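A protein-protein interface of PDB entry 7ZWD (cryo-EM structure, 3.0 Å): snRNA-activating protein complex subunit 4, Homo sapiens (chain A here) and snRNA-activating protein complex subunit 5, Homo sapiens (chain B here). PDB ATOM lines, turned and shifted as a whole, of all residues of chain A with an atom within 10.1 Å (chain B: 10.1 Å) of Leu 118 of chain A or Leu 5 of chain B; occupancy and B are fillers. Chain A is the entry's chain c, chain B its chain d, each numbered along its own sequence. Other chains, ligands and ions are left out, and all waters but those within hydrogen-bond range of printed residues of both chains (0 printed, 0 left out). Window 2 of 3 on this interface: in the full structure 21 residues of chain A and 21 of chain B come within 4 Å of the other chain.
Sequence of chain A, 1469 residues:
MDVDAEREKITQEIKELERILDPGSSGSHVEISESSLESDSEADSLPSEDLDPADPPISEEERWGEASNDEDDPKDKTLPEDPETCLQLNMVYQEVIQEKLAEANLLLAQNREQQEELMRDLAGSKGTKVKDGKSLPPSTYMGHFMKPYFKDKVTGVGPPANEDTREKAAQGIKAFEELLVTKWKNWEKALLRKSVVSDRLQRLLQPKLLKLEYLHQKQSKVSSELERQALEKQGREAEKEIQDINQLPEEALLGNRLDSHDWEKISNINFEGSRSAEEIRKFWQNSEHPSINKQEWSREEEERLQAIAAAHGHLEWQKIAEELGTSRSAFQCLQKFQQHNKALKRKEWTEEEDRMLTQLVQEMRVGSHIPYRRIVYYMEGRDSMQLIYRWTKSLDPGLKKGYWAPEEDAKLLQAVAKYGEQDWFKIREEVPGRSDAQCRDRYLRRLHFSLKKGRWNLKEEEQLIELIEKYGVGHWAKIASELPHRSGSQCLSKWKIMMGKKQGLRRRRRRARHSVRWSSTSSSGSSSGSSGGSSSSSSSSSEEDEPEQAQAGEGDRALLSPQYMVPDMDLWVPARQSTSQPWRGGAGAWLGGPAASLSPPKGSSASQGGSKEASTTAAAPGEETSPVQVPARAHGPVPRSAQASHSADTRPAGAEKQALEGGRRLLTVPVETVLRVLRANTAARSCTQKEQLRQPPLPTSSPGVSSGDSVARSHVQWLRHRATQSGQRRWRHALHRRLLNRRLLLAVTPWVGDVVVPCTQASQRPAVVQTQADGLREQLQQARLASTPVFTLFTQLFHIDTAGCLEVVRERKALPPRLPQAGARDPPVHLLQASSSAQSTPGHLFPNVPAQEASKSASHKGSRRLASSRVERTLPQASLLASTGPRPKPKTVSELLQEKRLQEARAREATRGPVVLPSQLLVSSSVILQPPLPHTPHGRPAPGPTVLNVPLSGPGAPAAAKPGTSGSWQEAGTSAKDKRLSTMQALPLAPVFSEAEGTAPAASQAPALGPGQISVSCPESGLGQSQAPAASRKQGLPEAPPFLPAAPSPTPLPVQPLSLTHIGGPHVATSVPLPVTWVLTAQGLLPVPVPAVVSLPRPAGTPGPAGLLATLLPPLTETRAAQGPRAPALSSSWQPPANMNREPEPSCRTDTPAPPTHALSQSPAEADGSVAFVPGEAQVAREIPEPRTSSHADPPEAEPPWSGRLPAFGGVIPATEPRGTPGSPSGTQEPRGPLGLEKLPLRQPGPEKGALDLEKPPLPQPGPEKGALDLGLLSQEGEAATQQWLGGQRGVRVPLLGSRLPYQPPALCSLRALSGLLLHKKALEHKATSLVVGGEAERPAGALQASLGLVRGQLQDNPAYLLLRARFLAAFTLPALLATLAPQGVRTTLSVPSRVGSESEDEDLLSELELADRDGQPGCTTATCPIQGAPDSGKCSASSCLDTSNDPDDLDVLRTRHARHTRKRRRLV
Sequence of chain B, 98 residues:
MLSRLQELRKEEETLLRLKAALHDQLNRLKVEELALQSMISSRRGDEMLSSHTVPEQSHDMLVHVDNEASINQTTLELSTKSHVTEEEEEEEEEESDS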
ATOM      1  N   GLN A 110     -13.624  -5.880  -8.547  1.00  0.00           N
ATOM      2  CA  GLN A 110     -12.340  -5.879  -7.854  1.00  0.00           C
ATOM      3  C   GLN A 110     -11.341  -6.808  -8.534  1.00  0.00           C
ATOM      4  O   GLN A 110     -10.156  -6.476  -8.653  1.00  0.00           O
ATOM      5  CB  GLN A 110     -12.519  -6.264  -6.384  1.00  0.00           C
ATOM      6  CG  GLN A 110     -13.433  -5.337  -5.590  1.00  0.00           C
ATOM      7  CD  GLN A 110     -14.138  -6.041  -4.442  1.00  0.00           C
ATOM      8  OE1 GLN A 110     -15.239  -6.567  -4.595  1.00  0.00           O
ATOM      9  NE2 GLN A 110     -13.498  -6.051  -3.279  1.00  0.00           N
ATOM     10  N   ASN A 111     -11.802  -7.965  -9.013  1.00  0.00           N
ATOM     11  CA  ASN A 111     -10.901  -8.899  -9.677  1.00  0.00           C
ATOM     12  C   ASN A 111     -10.440  -8.347 -11.019  1.00  0.00           C
ATOM     13  O   ASN A 111      -9.273  -8.500 -11.392  1.00  0.00           O
ATOM     14  CB  ASN A 111     -11.593 -10.252  -9.845  1.00  0.00           C
ATOM     15  CG  ASN A 111     -10.645 -11.353 -10.294  1.00  0.00           C
ATOM     16  OD1 ASN A 111      -9.524 -11.097 -10.731  1.00  0.00           O
ATOM     17  ND2 ASN A 111     -11.094 -12.594 -10.170  1.00  0.00           N
ATOM     18  N   ARG A 112     -11.332  -7.679 -11.752  1.00  0.00           N
ATOM     19  CA  ARG A 112     -10.945  -7.092 -13.030  1.00  0.00           C
ATOM     20  C   ARG A 112     -10.020  -5.903 -12.827  1.00  0.00           C
ATOM     21  O   ARG A 112      -9.129  -5.652 -13.646  1.00  0.00           O
ATOM     22  CB  ARG A 112     -12.188  -6.684 -13.821  1.00  0.00           C
ATOM     23  CG  ARG A 112     -13.028  -7.855 -14.305  1.00  0.00           C
ATOM     24  CD  ARG A 112     -12.159  -9.050 -14.649  1.00  0.00           C
ATOM     25  NE  ARG A 112     -12.921 -10.125 -15.273  1.00  0.00           N
ATOM     26  CZ  ARG A 112     -12.896 -10.401 -16.573  1.00  0.00           C
ATOM     27  NH1 ARG A 112     -12.141  -9.679 -17.392  1.00  0.00           N
ATOM     28  NH2 ARG A 112     -13.621 -11.400 -17.055  1.00  0.00           N
ATOM     29  N   GLU A 113     -10.204  -5.165 -11.730  1.00  0.00           N
ATOM     30  CA  GLU A 113      -9.256  -4.112 -11.389  1.00  0.00           C
ATOM     31  C   GLU A 113      -7.900  -4.702 -11.032  1.00  0.00           C
ATOM     32  O   GLU A 113      -6.859  -4.137 -11.381  1.00  0.00           O
ATOM     33  CB  GLU A 113      -9.795  -3.266 -10.236  1.00  0.00           C
ATOM     34  CG  GLU A 113      -8.906  -2.091  -9.824  1.00  0.00           C
ATOM     35  CD  GLU A 113      -8.317  -1.318 -10.999  1.00  0.00           C
ATOM     36  OE1 GLU A 113      -8.997  -1.173 -12.039  1.00  0.00           O
ATOM     37  OE2 GLU A 113      -7.164  -0.852 -10.883  1.00  0.00           O
ATOM     38  N   GLN A 114      -7.889  -5.841 -10.337  1.00  0.00           N
ATOM     39  CA  GLN A 114      -6.627  -6.524 -10.073  1.00  0.00           C
ATOM     40  C   GLN A 114      -5.972  -6.976 -11.371  1.00  0.00           C
ATOM     41  O   GLN A 114      -4.750  -6.879 -11.524  1.00  0.00           O
ATOM     42  CB  GLN A 114      -6.855  -7.709  -9.134  1.00  0.00           C
ATOM     43  CG  GLN A 114      -6.818  -7.337  -7.657  1.00  0.00           C
ATOM     44  CD  GLN A 114      -6.416  -8.497  -6.767  1.00  0.00           C
ATOM     45  OE1 GLN A 114      -5.423  -9.177  -7.025  1.00  0.00           O
ATOM     46  NE2 GLN A 114      -7.184  -8.726  -5.709  1.00  0.00           N
ATOM     47  N   GLN A 115      -6.775  -7.458 -12.321  1.00  0.00           N
ATOM     48  CA  GLN A 115      -6.237  -7.830 -13.625  1.00  0.00           C
ATOM     49  C   GLN A 115      -5.633  -6.624 -14.331  1.00  0.00           C
ATOM     50  O   GLN A 115      -4.541  -6.710 -14.901  1.00  0.00           O
ATOM     51  CB  GLN A 115      -7.330  -8.463 -14.489  1.00  0.00           C
ATOM     52  CG  GLN A 115      -7.964  -9.699 -13.884  1.00  0.00           C
ATOM     53  CD  GLN A 115      -6.960 -10.566 -13.158  1.00  0.00           C
ATOM     54  OE1 GLN A 115      -6.992 -10.680 -11.934  1.00  0.00           O
ATOM     55  NE2 GLN A 115      -6.059 -11.187 -13.910  1.00  0.00           N
ATOM     56  N   GLU A 116      -6.324  -5.485 -14.290  1.00  0.00           N
ATOM     57  CA  GLU A 116      -5.807  -4.286 -14.940  1.00  0.00           C
ATOM     58  C   GLU A 116      -4.552  -3.775 -14.239  1.00  0.00           C
ATOM     59  O   GLU A 116      -3.661  -3.209 -14.880  1.00  0.00           O
ATOM     60  CB  GLU A 116      -6.882  -3.203 -14.981  1.00  0.00           C
ATOM     61  CG  GLU A 116      -6.654  -2.159 -16.057  1.00  0.00           C
ATOM     62  CD  GLU A 116      -5.900  -0.954 -15.538  1.00  0.00           C
ATOM     63  OE1 GLU A 116      -4.894  -0.562 -16.165  1.00  0.00           O
ATOM     64  OE2 GLU A 116      -6.313  -0.400 -14.498  1.00  0.00           O
ATOM     65  N   GLU A 117      -4.462  -3.966 -12.921  1.00  0.00           N
ATOM     66  CA  GLU A 117      -3.234  -3.624 -12.209  1.00  0.00           C
ATOM     67  C   GLU A 117      -2.091  -4.533 -12.641  1.00  0.00           C
ATOM     68  O   GLU A 117      -0.953  -4.083 -12.817  1.00  0.00           O
ATOM     69  CB  GLU A 117      -3.456  -3.705 -10.697  1.00  0.00           C
ATOM     70  CG  GLU A 117      -4.284  -2.558 -10.133  1.00  0.00           C
ATOM     71  CD  GLU A 117      -5.058  -2.941  -8.886  1.00  0.00           C
ATOM     72  OE1 GLU A 117      -5.093  -4.141  -8.550  1.00  0.00           O
ATOM     73  OE2 GLU A 117      -5.629  -2.037  -8.240  1.00  0.00           O
ATOM     74  N   LEU A 118      -2.383  -5.819 -12.837  1.00  0.00           N
ATOM     75  CA  LEU A 118      -1.379  -6.728 -13.376  1.00  0.00           C
ATOM     76  C   LEU A 118      -0.912  -6.266 -14.752  1.00  0.00           C
ATOM     77  O   LEU A 118       0.289  -6.257 -15.044  1.00  0.00           O
ATOM     78  CB  LEU A 118      -1.941  -8.149 -13.439  1.00  0.00           C
ATOM     79  CG  LEU A 118      -2.365  -8.784 -12.112  1.00  0.00           C
ATOM     80  CD1 LEU A 118      -3.496  -9.773 -12.320  1.00  0.00           C
ATOM     81  CD2 LEU A 118      -1.186  -9.470 -11.443  1.00  0.00           C
ATOM     82  N   MET A 119      -1.853  -5.847 -15.603  1.00  0.00           N
ATOM     83  CA  MET A 119      -1.487  -5.413 -16.949  1.00  0.00           C
ATOM     84  C   MET A 119      -0.727  -4.091 -16.959  1.00  0.00           C
ATOM     85  O   MET A 119       0.162  -3.913 -17.797  1.00  0.00           O
ATOM     86  CB  MET A 119      -2.723  -5.299 -17.843  1.00  0.00           C
ATOM     87  CG  MET A 119      -3.697  -6.457 -17.738  1.00  0.00           C
ATOM     88  SD  MET A 119      -2.889  -8.069 -17.714  1.00  0.00           S
ATOM     89  CE  MET A 119      -4.158  -9.079 -16.949  1.00  0.00           C
ATOM     90  N   ARG A 120      -1.047  -3.161 -16.058  1.00  0.00           N
ATOM     91  CA  ARG A 120      -0.268  -1.928 -15.986  1.00  0.00           C
ATOM     92  C   ARG A 120       1.103  -2.185 -15.369  1.00  0.00           C
ATOM     93  O   ARG A 120       2.056  -1.442 -15.631  1.00  0.00           O
ATOM     94  CB  ARG A 120      -1.025  -0.852 -15.204  1.00  0.00           C
ATOM     95  CG  ARG A 120      -1.158  -1.117 -13.718  1.00  0.00           C
ATOM     96  CD  ARG A 120      -1.682   0.099 -12.971  1.00  0.00           C
ATOM     97  NE  ARG A 120      -1.980  -0.209 -11.575  1.00  0.00           N
ATOM     98  CZ  ARG A 120      -1.069  -0.267 -10.609  1.00  0.00           C
ATOM     99  NH1 ARG A 120       0.208  -0.045 -10.881  1.00  0.00           N
ATOM    100  NH2 ARG A 120      -1.436  -0.554  -9.370  1.00  0.00           N
ATOM    101  N   ASP A 121       1.220  -3.229 -14.541  1.00  0.00           N
ATOM    102  CA  ASP A 121       2.536  -3.689 -14.115  1.00  0.00           C
ATOM    103  C   ASP A 121       3.340  -4.220 -15.292  1.00  0.00           C
ATOM    104  O   ASP A 121       4.523  -3.887 -15.439  1.00  0.00           O
ATOM    105  CB  ASP A 121       2.390  -4.764 -13.035  1.00  0.00           C
ATOM    106  CG  ASP A 121       3.704  -5.462 -12.712  1.00  0.00           C
ATOM    107  OD1 ASP A 121       3.667  -6.662 -12.378  1.00  0.00           O
ATOM    108  OD2 ASP A 121       4.773  -4.822 -12.790  1.00  0.00           O
ATOM    109  N   LEU A 122       2.718  -5.044 -16.140  1.00  0.00           N
ATOM    110  CA  LEU A 122       3.405  -5.506 -17.345  1.00  0.00           C
ATOM    111  C   LEU A 122       3.756  -4.344 -18.268  1.00  0.00           C
ATOM    112  O   LEU A 122       4.755  -4.411 -18.994  1.00  0.00           O
ATOM    113  CB  LEU A 122       2.553  -6.532 -18.095  1.00  0.00           C
ATOM    114  CG  LEU A 122       1.803  -7.595 -17.294  1.00  0.00           C
ATOM    115  CD1 LEU A 122       0.875  -8.392 -18.196  1.00  0.00           C
ATOM    116  CD2 LEU A 122       2.772  -8.511 -16.566  1.00  0.00           C
ATOM    117  N   ALA A 123       2.959  -3.273 -18.247  1.00  0.00           N
ATOM    118  CA  ALA A 123       3.194  -2.105 -19.087  1.00  0.00           C
ATOM    119  C   ALA A 123       3.842  -0.954 -18.327  1.00  0.00           C
ATOM    120  O   ALA A 123       3.790   0.189 -18.795  1.00  0.00           O
ATOM    121  CB  ALA A 123       1.885  -1.639 -19.729  1.00  0.00           C
ATOM    122  N   GLY A 124       4.441  -1.219 -17.167  1.00  0.00           N
ATOM    123  CA  GLY A 124       5.157  -0.196 -16.426  1.00  0.00           C
ATOM    124  C   GLY A 124       6.637  -0.143 -16.751  1.00  0.00           C
ATOM    125  O   GLY A 124       7.195  -1.111 -17.276  1.00  0.00           O
ATOM    126  N   MET B   1       4.686 -13.822 -10.635  1.00  0.00           N
ATOM    127  CA  MET B   1       3.374 -13.466 -10.107  1.00  0.00           C
ATOM    128  C   MET B   1       2.279 -14.231 -10.830  1.00  0.00           C
ATOM    129  O   MET B   1       1.096 -14.088 -10.518  1.00  0.00           O
ATOM    130  CB  MET B   1       3.131 -11.964 -10.235  1.00  0.00           C
ATOM    131  CG  MET B   1       3.093 -11.464 -11.664  1.00  0.00           C
ATOM    132  SD  MET B   1       3.288  -9.678 -11.740  1.00  0.00           S
ATOM    133  CE  MET B   1       2.290  -9.171 -10.343  1.00  0.00           C
ATOM    134  N   LEU B   2       2.684 -15.049 -11.804  1.00  0.00           N
ATOM    135  CA  LEU B   2       1.701 -15.793 -12.582  1.00  0.00           C
ATOM    136  C   LEU B   2       0.971 -16.819 -11.729  1.00  0.00           C
ATOM    137  O   LEU B   2      -0.149 -17.202 -12.061  1.00  0.00           O
ATOM    138  CB  LEU B   2       2.361 -16.483 -13.774  1.00  0.00           C
ATOM    139  CG  LEU B   2       2.319 -15.790 -15.136  1.00  0.00           C
ATOM    140  CD1 LEU B   2       3.030 -16.648 -16.169  1.00  0.00           C
ATOM    141  CD2 LEU B   2       0.902 -15.471 -15.569  1.00  0.00           C
ATOM    142  N   SER B   3       1.590 -17.297 -10.647  1.00  0.00           N
ATOM    143  CA  SER B   3       0.870 -18.172  -9.727  1.00  0.00           C
ATOM    144  C   SER B   3      -0.348 -17.462  -9.153  1.00  0.00           C
ATOM    145  O   SER B   3      -1.480 -17.957  -9.252  1.00  0.00           O
ATOM    146  CB  SER B   3       1.798 -18.630  -8.600  1.00  0.00           C
ATOM    147  OG  SER B   3       2.632 -19.700  -9.009  1.00  0.00           O
ATOM    148  N   ARG B   4      -0.130 -16.287  -8.561  1.00  0.00           N
ATOM    149  CA  ARG B   4      -1.240 -15.489  -8.066  1.00  0.00           C
ATOM    150  C   ARG B   4      -2.169 -15.081  -9.201  1.00  0.00           C
ATOM    151  O   ARG B   4      -3.391 -15.071  -9.031  1.00  0.00           O
ATOM    152  CB  ARG B   4      -0.715 -14.258  -7.331  1.00  0.00           C
ATOM    153  CG  ARG B   4      -1.789 -13.485  -6.591  1.00  0.00           C
ATOM    154  CD  ARG B   4      -2.466 -14.355  -5.547  1.00  0.00           C
ATOM    155  NE  ARG B   4      -3.844 -14.667  -5.911  1.00  0.00           N
ATOM    156  CZ  ARG B   4      -4.659 -15.408  -5.170  1.00  0.00           C
ATOM    157  NH1 ARG B   4      -4.233 -15.915  -4.022  1.00  0.00           N
ATOM    158  NH2 ARG B   4      -5.897 -15.647  -5.577  1.00  0.00           N
ATOM    159  N   LEU B   5      -1.610 -14.747 -10.366  1.00  0.00           N
ATOM    160  CA  LEU B   5      -2.441 -14.323 -11.487  1.00  0.00           C
ATOM    161  C   LEU B   5      -3.399 -15.434 -11.909  1.00  0.00           C
ATOM    162  O   LEU B   5      -4.578 -15.179 -12.192  1.00  0.00           O
ATOM    163  CB  LEU B   5      -1.549 -13.885 -12.651  1.00  0.00           C
ATOM    164  CG  LEU B   5      -2.166 -13.136 -13.836  1.00  0.00           C
ATOM    165  CD1 LEU B   5      -1.140 -12.195 -14.459  1.00  0.00           C
ATOM    166  CD2 LEU B   5      -2.703 -14.094 -14.888  1.00  0.00           C
ATOM    167  N   GLN B   6      -2.921 -16.679 -11.925  1.00  0.00           N
ATOM    168  CA  GLN B   6      -3.778 -17.789 -12.323  1.00  0.00           C
ATOM    169  C   GLN B   6      -4.766 -18.147 -11.227  1.00  0.00           C
ATOM    170  O   GLN B   6      -5.904 -18.532 -11.516  1.00  0.00           O
ATOM    171  CB  GLN B   6      -2.940 -19.007 -12.708  1.00  0.00           C
ATOM    172  CG  GLN B   6      -1.960 -18.761 -13.846  1.00  0.00           C
ATOM    173  CD  GLN B   6      -2.566 -18.015 -15.021  1.00  0.00           C
ATOM    174  OE1 GLN B   6      -3.741 -18.175 -15.345  1.00  0.00           O
ATOM    175  NE2 GLN B   6      -1.757 -17.196 -15.670  1.00  0.00           N
ATOM    176  N   GLU B   7      -4.362 -18.019  -9.963  1.00  0.00           N
ATOM    177  CA  GLU B   7      -5.329 -18.187  -8.884  1.00  0.00           C
ATOM    178  C   GLU B   7      -6.468 -17.184  -9.026  1.00  0.00           C
ATOM    179  O   GLU B   7      -7.651 -17.542  -8.928  1.00  0.00           O
ATOM    180  CB  GLU B   7      -4.635 -18.047  -7.530  1.00  0.00           C
ATOM    181  CG  GLU B   7      -4.079 -19.359  -6.990  1.00  0.00           C
ATOM    182  CD  GLU B   7      -3.483 -19.222  -5.604  1.00  0.00           C
ATOM    183  OE1 GLU B   7      -3.022 -20.241  -5.050  1.00  0.00           O
ATOM    184  OE2 GLU B   7      -3.468 -18.097  -5.067  1.00  0.00           O
ATOM    185  N   LEU B   8      -6.126 -15.921  -9.296  1.00  0.00           N
ATOM    186  CA  LEU B   8      -7.148 -14.889  -9.442  1.00  0.00           C
ATOM    187  C   LEU B   8      -8.028 -15.135 -10.663  1.00  0.00           C
ATOM    188  O   LEU B   8      -9.247 -14.949 -10.596  1.00  0.00           O
ATOM    189  CB  LEU B   8      -6.508 -13.502  -9.518  1.00  0.00           C
ATOM    190  CG  LEU B   8      -5.554 -13.053  -8.408  1.00  0.00           C
ATOM    191  CD1 LEU B   8      -4.729 -11.856  -8.862  1.00  0.00           C
ATOM    192  CD2 LEU B   8      -6.314 -12.733  -7.131  1.00  0.00           C
ATOM    193  N   ARG B   9      -7.440 -15.564 -11.786  1.00  0.00           N
ATOM    194  CA  ARG B   9      -8.265 -15.802 -12.969  1.00  0.00           C
ATOM    195  C   ARG B   9      -9.180 -17.004 -12.765  1.00  0.00           C
ATOM    196  O   ARG B   9     -10.302 -17.028 -13.281  1.00  0.00           O
ATOM    197  CB  ARG B   9      -7.401 -15.993 -14.221  1.00  0.00           C
ATOM    198  CG  ARG B   9      -6.527 -17.222 -14.198  1.00  0.00           C
ATOM    199  CD  ARG B   9      -7.248 -18.457 -14.756  1.00  0.00           C
ATOM    200  NE  ARG B   9      -6.514 -19.696 -14.526  1.00  0.00           N
ATOM    201  CZ  ARG B   9      -7.049 -20.907 -14.640  1.00  0.00           C
ATOM    202  NH1 ARG B   9      -8.328 -21.030 -14.977  1.00  0.00           N
ATOM    203  NH2 ARG B   9      -6.314 -21.988 -14.407  1.00  0.00           N
ATOM    204  N   LYS B  10      -8.707 -18.031 -12.052  1.00  0.00           N
ATOM    205  CA  LYS B  10      -9.553 -19.191 -11.794  1.00  0.00           C
ATOM    206  C   LYS B  10     -10.718 -18.808 -10.899  1.00  0.00           C
ATOM    207  O   LYS B  10     -11.864 -19.217 -11.137  1.00  0.00           O
ATOM    208  CB  LYS B  10      -8.736 -20.311 -11.158  1.00  0.00           C
ATOM    209  CG  LYS B  10      -9.582 -21.477 -10.673  1.00  0.00           C
ATOM    210  CD  LYS B  10     -10.339 -22.137 -11.815  1.00  0.00           C
ATOM    211  CE  LYS B  10     -11.219 -23.268 -11.313  1.00  0.00           C
ATOM    212  NZ  LYS B  10     -11.968 -23.914 -12.421  1.00  0.00           N
ATOM    213  N   GLU B  11     -10.439 -18.021  -9.858  1.00  0.00           N
ATOM    214  CA  GLU B  11     -11.523 -17.423  -9.094  1.00  0.00           C
ATOM    215  C   GLU B  11     -12.459 -16.628  -9.992  1.00  0.00           C
ATOM    216  O   GLU B  11     -13.678 -16.659  -9.794  1.00  0.00           O
ATOM    217  CB  GLU B  11     -10.958 -16.527  -7.994  1.00  0.00           C
ATOM    218  CG  GLU B  11     -10.542 -17.277  -6.750  1.00  0.00           C
ATOM    219  CD  GLU B  11     -10.845 -16.502  -5.490  1.00  0.00           C
ATOM    220  OE1 GLU B  11     -10.258 -15.417  -5.299  1.00  0.00           O
ATOM    221  OE2 GLU B  11     -11.693 -16.968  -4.704  1.00  0.00           O
ATOM    222  N   GLU B  12     -11.910 -15.937 -10.992  1.00  0.00           N
ATOM    223  CA  GLU B  12     -12.730 -15.122 -11.880  1.00  0.00           C
ATOM    224  C   GLU B  12     -13.682 -15.987 -12.695  1.00  0.00           C
ATOM    225  O   GLU B  12     -14.865 -15.665 -12.835  1.00  0.00           O
ATOM    226  CB  GLU B  12     -11.830 -14.291 -12.794  1.00  0.00           C
ATOM    227  CG  GLU B  12     -12.559 -13.313 -13.687  1.00  0.00           C
ATOM    228  CD  GLU B  12     -11.708 -12.868 -14.855  1.00  0.00           C
ATOM    229  OE1 GLU B  12     -11.901 -13.395 -15.968  1.00  0.00           O
ATOM    230  OE2 GLU B  12     -10.841 -11.992 -14.658  1.00  0.00           O
ATOM    231  N   GLU B  13     -13.179 -17.089 -13.247  1.00  0.00           N
ATOM    232  CA  GLU B  13     -14.041 -17.979 -14.024  1.00  0.00           C
ATOM    233  C   GLU B  13     -15.086 -18.641 -13.136  1.00  0.00           C
ATOM    234  O   GLU B  13     -16.242 -18.809 -13.544  1.00  0.00           O
ATOM    235  CB  GLU B  13     -13.211 -19.034 -14.758  1.00  0.00           C
ATOM    236  CG  GLU B  13     -11.904 -18.535 -15.366  1.00  0.00           C
ATOM    237  CD  GLU B  13     -12.044 -17.248 -16.173  1.00  0.00           C
ATOM    238  OE1 GLU B  13     -11.037 -16.517 -16.287  1.00  0.00           O
ATOM    239  OE2 GLU B  13     -13.132 -16.981 -16.726  1.00  0.00           O
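Among the printed residues, merely in contact across the chains: Asn 111 of chain A with Glu 12 of chain B (3.2 Å), Gln 114 of chain A with Leu 8 of chain B (3.3 Å), Leu 118 of chain A with Met 1 of chain B (3.7 Å), Gln 115 of chain A with Leu 8 of chain B (3.7 Å), Gln 115 of chain A with Glu 12 of chain B (3.8 Å) and Leu 118 of chain A with Leu 5 of chain B (3.9 Å).
The side-chain amide oxygen (OD1) of Asn 111 of chain A sits close to the side-chain amide oxygen (OE1) of Gln 115 of chain A.
The side-chain amide nitrogen (ND2) of Asn 111 of chain A lies within hydrogen-bond range of the backbone carbonyl oxygen (O) of Leu 8 of chain B. NH2 of Arg 112 of chain A is in salt-bridge range of OE1 of Glu 12 of chain B, at 2.8 Å. SD of Met 1 of chain B lies close to OD1 of Asp 121 of chain A (3.1 Å).
Of the printed residues of chain B, Asn 111 of chain A touches Leu 8 and Glu 12. Printed residues of chain B within 4 Å of Arg 112 of chain A: Glu 12. Of the printed residues of chain B, Gln 114 of chain A touches Leu 8 (3.3 Å). Of the printed residues of chain B, Leu 118 of chain A touches Met 1 and Leu 5. No residue of chain B comes within 4 Å of Met 119 of chain A. Printed residues of chain A within 4 Å of Met 1 of chain B: Leu 118 and Asp 121. Leu 5 of chain B touches just one residue of chain A: Leu 118 (3.9 Å). No residue of chain A comes within 4 Å of Gln 6 of chain B. Printed residues of chain A within 4 Å of Glu 12 of chain B: Asn 111, Arg 112 and Gln 115.
Of the 15 printed residues of chain A, 6 touch a printed residue of chain B. Of the 13 printed residues of chain B, 4 touch a printed residue of chain A. Printed residues of chain B that touch a printed residue of chain A: Met 1, Leu 5, Leu 8 and Glu 12. Hydrophobic or aromatic side chains of chain B that line the printed part of chain A: Met 1, Leu 5 and Leu 8.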
